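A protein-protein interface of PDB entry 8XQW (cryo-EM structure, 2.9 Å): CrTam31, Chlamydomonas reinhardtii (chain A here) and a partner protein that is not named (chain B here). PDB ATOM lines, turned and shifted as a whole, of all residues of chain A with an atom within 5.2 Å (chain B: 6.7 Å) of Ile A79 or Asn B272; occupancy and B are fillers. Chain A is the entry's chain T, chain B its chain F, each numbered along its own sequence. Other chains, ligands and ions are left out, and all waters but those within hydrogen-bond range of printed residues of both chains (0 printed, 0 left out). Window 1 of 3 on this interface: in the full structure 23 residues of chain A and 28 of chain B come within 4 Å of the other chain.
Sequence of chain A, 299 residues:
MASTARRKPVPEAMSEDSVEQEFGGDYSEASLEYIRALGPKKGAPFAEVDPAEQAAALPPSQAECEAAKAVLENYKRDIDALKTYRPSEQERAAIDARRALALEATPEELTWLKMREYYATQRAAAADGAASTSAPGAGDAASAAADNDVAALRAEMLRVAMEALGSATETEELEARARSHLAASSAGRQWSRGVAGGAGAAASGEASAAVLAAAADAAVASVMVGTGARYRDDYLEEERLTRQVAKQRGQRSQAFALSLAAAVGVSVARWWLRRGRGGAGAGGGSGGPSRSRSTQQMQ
NZ of Lys A76 is in hydrogen-bond range of OH of Tyr B273.
The backbone carbonyl oxygen (O) of Ala B266 lies within hydrogen-bond range of the side-chain amino group (NZ) of Lys A83 (2.7 Å).
The side-chain carboxylate (OD2) of Asp B270 is in salt-bridge range of the side-chain amino group (NZ) of Lys A83 (3.96 Å).
Among the printed residues, pairs that only touch across the chains: Ile A79 with Leu B269, Ile A79 with Asn B272, Leu A82 with Leu B269, Ile A79 with Tyr B273 and Lys A83 with Leu B269.
Of the 10 printed residues of chain A, 4 touch a printed residue of chain B.
Hydrophobic or aromatic side chains of chain A that line the printed part of chain B: Ile A79 and Leu A82.
Along chain A the printed residues that touch a printed residue of chain B span positions 76 to 83.
Of the 12 printed residues of chain B, 5 touch a printed residue of chain A.
Hydrophobic or aromatic side chains of chain B that line the printed part of chain A: Ala B266, Leu B269 and Tyr B273.
Among the printed residues, Asp or Glu carboxylates within 4 Å of a Lys or Arg side-chain nitrogen of the other chain: Lys A83 with Asp B270 (3.96 Å).
The side-chain carboxylate (OD1) of Asp A80 sits close to the backbone carbonyl oxygen (O) of Lys A76 (2.7 Å).
Of the printed residues of chain B, Lys A76 touches Tyr B273 (3.0 Å).
Of the printed residues of chain B, Ile A79 touches Leu B269, Asn B272 and Tyr B273.
Of the printed residues of chain B, Leu A82 touches Leu B269 (3.5 Å).
Printed residues of chain A within 4 Å of Leu B269: Ile A79 (3.2 Å), Leu A82 (3.5 Å) and Lys A83 (3.9 Å).
Of chain A, only Ile A79 comes within 4 Å of Asn B272.
Of the printed residues of chain A, Tyr B273 touches Lys A76 (3.0 Å) and Ile A79 (3.6 Å).
The nearest printed residue of chain B that does not touch Lys A76 is Ala B277 (6.9 Å).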
ATOM      1  N   ASN A  74      -6.788  -5.924 -25.098  1.00  0.00           N
ATOM      2  CA  ASN A  74      -6.893  -4.616 -25.739  1.00  0.00           C
ATOM      3  C   ASN A  74      -8.301  -4.373 -26.271  1.00  0.00           C
ATOM      4  O   ASN A  74      -8.831  -3.260 -26.168  1.00  0.00           O
ATOM      5  CB  ASN A  74      -5.873  -4.504 -26.868  1.00  0.00           C
ATOM      6  CG  ASN A  74      -5.841  -3.130 -27.479  1.00  0.00           C
ATOM      7  OD1 ASN A  74      -5.912  -2.127 -26.770  1.00  0.00           O
ATOM      8  ND2 ASN A  74      -5.745  -3.067 -28.801  1.00  0.00           N
ATOM      9  N   TYR A  75      -8.915  -5.407 -26.843  1.00  0.00           N
ATOM     10  CA  TYR A  75     -10.233  -5.262 -27.443  1.00  0.00           C
ATOM     11  C   TYR A  75     -11.288  -4.945 -26.398  1.00  0.00           C
ATOM     12  O   TYR A  75     -12.129  -4.069 -26.612  1.00  0.00           O
ATOM     13  CB  TYR A  75     -10.601  -6.528 -28.211  1.00  0.00           C
ATOM     14  CG  TYR A  75     -10.191  -6.503 -29.662  1.00  0.00           C
ATOM     15  CD1 TYR A  75      -9.883  -5.307 -30.296  1.00  0.00           C
ATOM     16  CD2 TYR A  75     -10.134  -7.672 -30.408  1.00  0.00           C
ATOM     17  CE1 TYR A  75      -9.513  -5.279 -31.629  1.00  0.00           C
ATOM     18  CE2 TYR A  75      -9.767  -7.655 -31.744  1.00  0.00           C
ATOM     19  CZ  TYR A  75      -9.457  -6.455 -32.349  1.00  0.00           C
ATOM     20  OH  TYR A  75      -9.093  -6.430 -33.676  1.00  0.00           O
ATOM     21  N   LYS A  76     -11.275  -5.650 -25.266  1.00  0.00           N
ATOM     22  CA  LYS A  76     -12.232  -5.324 -24.211  1.00  0.00           C
ATOM     23  C   LYS A  76     -11.978  -3.921 -23.669  1.00  0.00           C
ATOM     24  O   LYS A  76     -12.924  -3.177 -23.377  1.00  0.00           O
ATOM     25  CB  LYS A  76     -12.202  -6.357 -23.080  1.00  0.00           C
ATOM     26  CG  LYS A  76     -10.833  -6.775 -22.613  1.00  0.00           C
ATOM     27  CD  LYS A  76     -10.841  -8.172 -22.026  1.00  0.00           C
ATOM     28  CE  LYS A  76     -11.901  -8.306 -20.947  1.00  0.00           C
ATOM     29  NZ  LYS A  76     -11.601  -9.410 -19.992  1.00  0.00           N
ATOM     30  N   ARG A  77     -10.703  -3.538 -23.532  1.00  0.00           N
ATOM     31  CA  ARG A  77     -10.396  -2.182 -23.079  1.00  0.00           C
ATOM     32  C   ARG A  77     -11.022  -1.140 -24.001  1.00  0.00           C
ATOM     33  O   ARG A  77     -11.732  -0.237 -23.545  1.00  0.00           O
ATOM     34  CB  ARG A  77      -8.885  -1.972 -22.987  1.00  0.00           C
ATOM     35  CG  ARG A  77      -8.170  -2.890 -22.010  1.00  0.00           C
ATOM     36  CD  ARG A  77      -6.706  -2.507 -21.877  1.00  0.00           C
ATOM     37  NE  ARG A  77      -5.817  -3.593 -22.277  1.00  0.00           N
ATOM     38  CZ  ARG A  77      -4.934  -3.502 -23.265  1.00  0.00           C
ATOM     39  NH1 ARG A  77      -4.824  -2.373 -23.951  1.00  0.00           N
ATOM     40  NH2 ARG A  77      -4.166  -4.537 -23.574  1.00  0.00           N
ATOM     41  N   ASP A  78     -10.786  -1.261 -25.308  1.00  0.00           N
ATOM     42  CA  ASP A  78     -11.330  -0.265 -26.227  1.00  0.00           C
ATOM     43  C   ASP A  78     -12.838  -0.407 -26.413  1.00  0.00           C
ATOM     44  O   ASP A  78     -13.501   0.568 -26.776  1.00  0.00           O
ATOM     45  CB  ASP A  78     -10.611  -0.316 -27.575  1.00  0.00           C
ATOM     46  CG  ASP A  78      -9.128  -0.016 -27.455  1.00  0.00           C
ATOM     47  OD1 ASP A  78      -8.754   1.172 -27.557  1.00  0.00           O
ATOM     48  OD2 ASP A  78      -8.336  -0.955 -27.270  1.00  0.00           O
ATOM     49  N   ILE A  79     -13.410  -1.581 -26.143  1.00  0.00           N
ATOM     50  CA  ILE A  79     -14.863  -1.712 -26.225  1.00  0.00           C
ATOM     51  C   ILE A  79     -15.529  -0.975 -25.073  1.00  0.00           C
ATOM     52  O   ILE A  79     -16.517  -0.260 -25.267  1.00  0.00           O
ATOM     53  CB  ILE A  79     -15.275  -3.194 -26.279  1.00  0.00           C
ATOM     54  CG1 ILE A  79     -15.085  -3.733 -27.698  1.00  0.00           C
ATOM     55  CG2 ILE A  79     -16.715  -3.369 -25.825  1.00  0.00           C
ATOM     56  CD1 ILE A  79     -15.428  -5.191 -27.862  1.00  0.00           C
ATOM     57  N   ASP A  80     -14.986  -1.104 -23.860  1.00  0.00           N
ATOM     58  CA  ASP A  80     -15.500  -0.283 -22.766  1.00  0.00           C
ATOM     59  C   ASP A  80     -15.165   1.196 -22.961  1.00  0.00           C
ATOM     60  O   ASP A  80     -15.925   2.071 -22.522  1.00  0.00           O
ATOM     61  CB  ASP A  80     -14.975  -0.804 -21.428  1.00  0.00           C
ATOM     62  CG  ASP A  80     -15.369  -2.252 -21.172  1.00  0.00           C
ATOM     63  OD1 ASP A  80     -15.251  -3.087 -22.092  1.00  0.00           O
ATOM     64  OD2 ASP A  80     -15.804  -2.558 -20.045  1.00  0.00           O
ATOM     65  N   ALA A  81     -14.049   1.495 -23.635  1.00  0.00           N
ATOM     66  CA  ALA A  81     -13.739   2.877 -23.987  1.00  0.00           C
ATOM     67  C   ALA A  81     -14.813   3.464 -24.900  1.00  0.00           C
ATOM     68  O   ALA A  81     -15.306   4.573 -24.666  1.00  0.00           O
ATOM     69  CB  ALA A  81     -12.364   2.952 -24.653  1.00  0.00           C
ATOM     70  N   LEU A  82     -15.178   2.731 -25.953  1.00  0.00           N
ATOM     71  CA  LEU A  82     -16.314   3.096 -26.787  1.00  0.00           C
ATOM     72  C   LEU A  82     -17.590   3.219 -25.968  1.00  0.00           C
ATOM     73  O   LEU A  82     -18.383   4.135 -26.206  1.00  0.00           O
ATOM     74  CB  LEU A  82     -16.487   2.052 -27.896  1.00  0.00           C
ATOM     75  CG  LEU A  82     -17.343   2.305 -29.143  1.00  0.00           C
ATOM     76  CD1 LEU A  82     -18.832   2.367 -28.835  1.00  0.00           C
ATOM     77  CD2 LEU A  82     -16.879   3.569 -29.856  1.00  0.00           C
ATOM     78  N   LYS A  83     -17.796   2.310 -25.014  1.00  0.00           N
ATOM     79  CA  LYS A  83     -18.919   2.426 -24.093  1.00  0.00           C
ATOM     80  C   LYS A  83     -18.937   3.786 -23.411  1.00  0.00           C
ATOM     81  O   LYS A  83     -20.012   4.348 -23.171  1.00  0.00           O
ATOM     82  CB  LYS A  83     -18.851   1.308 -23.051  1.00  0.00           C
ATOM     83  CG  LYS A  83     -20.186   0.843 -22.509  1.00  0.00           C
ATOM     84  CD  LYS A  83     -19.982  -0.025 -21.272  1.00  0.00           C
ATOM     85  CE  LYS A  83     -19.349  -1.368 -21.612  1.00  0.00           C
ATOM     86  NZ  LYS A  83     -20.341  -2.305 -22.202  1.00  0.00           N
ATOM     87  N   ALA B 266     -24.201  -0.096 -23.794  1.00  0.00           N
ATOM     88  CA  ALA B 266     -23.341  -0.929 -22.963  1.00  0.00           C
ATOM     89  C   ALA B 266     -23.596  -2.407 -23.214  1.00  0.00           C
ATOM     90  O   ALA B 266     -22.649  -3.193 -23.336  1.00  0.00           O
ATOM     91  CB  ALA B 266     -23.552  -0.592 -21.487  1.00  0.00           C
ATOM     92  N   ALA B 267     -24.871  -2.801 -23.293  1.00  0.00           N
ATOM     93  CA  ALA B 267     -25.203  -4.206 -23.494  1.00  0.00           C
ATOM     94  C   ALA B 267     -24.567  -4.743 -24.770  1.00  0.00           C
ATOM     95  O   ALA B 267     -23.868  -5.766 -24.753  1.00  0.00           O
ATOM     96  CB  ALA B 267     -26.723  -4.381 -23.528  1.00  0.00           C
ATOM     97  N   ALA B 268     -24.801  -4.054 -25.891  1.00  0.00           N
ATOM     98  CA  ALA B 268     -24.284  -4.495 -27.179  1.00  0.00           C
ATOM     99  C   ALA B 268     -22.764  -4.471 -27.208  1.00  0.00           C
ATOM    100  O   ALA B 268     -22.136  -5.389 -27.742  1.00  0.00           O
ATOM    101  CB  ALA B 268     -24.854  -3.620 -28.294  1.00  0.00           C
ATOM    102  N   LEU B 269     -22.148  -3.441 -26.631  1.00  0.00           N
ATOM    103  CA  LEU B 269     -20.693  -3.386 -26.657  1.00  0.00           C
ATOM    104  C   LEU B 269     -20.098  -4.563 -25.893  1.00  0.00           C
ATOM    105  O   LEU B 269     -19.225  -5.283 -26.404  1.00  0.00           O
ATOM    106  CB  LEU B 269     -20.212  -2.050 -26.087  1.00  0.00           C
ATOM    107  CG  LEU B 269     -20.014  -0.903 -27.086  1.00  0.00           C
ATOM    108  CD1 LEU B 269     -18.651  -1.003 -27.737  1.00  0.00           C
ATOM    109  CD2 LEU B 269     -21.110  -0.869 -28.149  1.00  0.00           C
ATOM    110  N   ASP B 270     -20.602  -4.815 -24.684  1.00  0.00           N
ATOM    111  CA  ASP B 270     -19.983  -5.852 -23.869  1.00  0.00           C
ATOM    112  C   ASP B 270     -20.302  -7.247 -24.390  1.00  0.00           C
ATOM    113  O   ASP B 270     -19.452  -8.136 -24.306  1.00  0.00           O
ATOM    114  CB  ASP B 270     -20.387  -5.689 -22.396  1.00  0.00           C
ATOM    115  CG  ASP B 270     -21.760  -6.267 -22.075  1.00  0.00           C
ATOM    116  OD1 ASP B 270     -21.919  -7.505 -22.091  1.00  0.00           O
ATOM    117  OD2 ASP B 270     -22.678  -5.474 -21.781  1.00  0.00           O
ATOM    118  N   ASP B 271     -21.488  -7.473 -24.965  1.00  0.00           N
ATOM    119  CA  ASP B 271     -21.756  -8.827 -25.444  1.00  0.00           C
ATOM    120  C   ASP B 271     -21.124  -9.054 -26.813  1.00  0.00           C
ATOM    121  O   ASP B 271     -20.861 -10.198 -27.198  1.00  0.00           O
ATOM    122  CB  ASP B 271     -23.262  -9.127 -25.445  1.00  0.00           C
ATOM    123  CG  ASP B 271     -24.046  -8.288 -26.428  1.00  0.00           C
ATOM    124  OD1 ASP B 271     -23.458  -7.421 -27.086  1.00  0.00           O
ATOM    125  OD2 ASP B 271     -25.274  -8.489 -26.524  1.00  0.00           O
ATOM    126  N   ASN B 272     -20.818  -7.982 -27.549  1.00  0.00           N
ATOM    127  CA  ASN B 272     -19.943  -8.121 -28.708  1.00  0.00           C
ATOM    128  C   ASN B 272     -18.548  -8.556 -28.276  1.00  0.00           C
ATOM    129  O   ASN B 272     -17.940  -9.458 -28.880  1.00  0.00           O
ATOM    130  CB  ASN B 272     -19.895  -6.801 -29.479  1.00  0.00           C
ATOM    131  CG  ASN B 272     -18.750  -6.739 -30.464  1.00  0.00           C
ATOM    132  OD1 ASN B 272     -17.688  -6.188 -30.172  1.00  0.00           O
ATOM    133  ND2 ASN B 272     -18.960  -7.300 -31.649  1.00  0.00           N
ATOM    134  N   TYR B 273     -18.021  -7.921 -27.223  1.00  0.00           N
ATOM    135  CA  TYR B 273     -16.790  -8.428 -26.620  1.00  0.00           C
ATOM    136  C   TYR B 273     -16.937  -9.894 -26.228  1.00  0.00           C
ATOM    137  O   TYR B 273     -16.010 -10.691 -26.411  1.00  0.00           O
ATOM    138  CB  TYR B 273     -16.398  -7.602 -25.396  1.00  0.00           C
ATOM    139  CG  TYR B 273     -15.678  -8.439 -24.361  1.00  0.00           C
ATOM    140  CD1 TYR B 273     -14.367  -8.850 -24.559  1.00  0.00           C
ATOM    141  CD2 TYR B 273     -16.328  -8.856 -23.208  1.00  0.00           C
ATOM    142  CE1 TYR B 273     -13.718  -9.636 -23.628  1.00  0.00           C
ATOM    143  CE2 TYR B 273     -15.688  -9.640 -22.271  1.00  0.00           C
ATOM    144  CZ  TYR B 273     -14.382 -10.027 -22.485  1.00  0.00           C
ATOM    145  OH  TYR B 273     -13.736 -10.808 -21.552  1.00  0.00           O
ATOM    146  N   GLN B 274     -18.088 -10.253 -25.659  1.00  0.00           N
ATOM    147  CA  GLN B 274     -18.338 -11.634 -25.263  1.00  0.00           C
ATOM    148  C   GLN B 274     -18.267 -12.573 -26.459  1.00  0.00           C
ATOM    149  O   GLN B 274     -17.744 -13.687 -26.353  1.00  0.00           O
ATOM    150  CB  GLN B 274     -19.702 -11.731 -24.578  1.00  0.00           C
ATOM    151  CG  GLN B 274     -20.224 -13.143 -24.404  1.00  0.00           C
ATOM    152  CD  GLN B 274     -21.289 -13.493 -25.424  1.00  0.00           C
ATOM    153  OE1 GLN B 274     -21.812 -12.618 -26.115  1.00  0.00           O
ATOM    154  NE2 GLN B 274     -21.614 -14.774 -25.525  1.00  0.00           N
ATOM    155  N   ALA B 275     -18.778 -12.132 -27.609  1.00  0.00           N
ATOM    156  CA  ALA B 275     -18.725 -12.947 -28.818  1.00  0.00           C
ATOM    157  C   ALA B 275     -17.286 -13.164 -29.273  1.00  0.00           C
ATOM    158  O   ALA B 275     -16.882 -14.292 -29.593  1.00  0.00           O
ATOM    159  CB  ALA B 275     -19.545 -12.285 -29.925  1.00  0.00           C
ATOM    160  N   ALA B 276     -16.501 -12.086 -29.323  1.00  0.00           N
ATOM    161  CA  ALA B 276     -15.100 -12.228 -29.717  1.00  0.00           C
ATOM    162  C   ALA B 276     -14.350 -13.140 -28.752  1.00  0.00           C
ATOM    163  O   ALA B 276     -13.541 -13.987 -29.169  1.00  0.00           O
ATOM    164  CB  ALA B 276     -14.430 -10.857 -29.795  1.00  0.00           C
ATOM    165  N   ALA B 277     -14.613 -12.980 -27.455  1.00  0.00           N
ATOM    166  CA  ALA B 277     -13.974 -13.819 -26.451  1.00  0.00           C
ATOM    167  C   ALA B 277     -14.380 -15.276 -26.615  1.00  0.00           C
ATOM    168  O   ALA B 277     -13.550 -16.174 -26.460  1.00  0.00           O
ATOM    169  CB  ALA B 277     -14.318 -13.316 -25.051  1.00  0.00           C
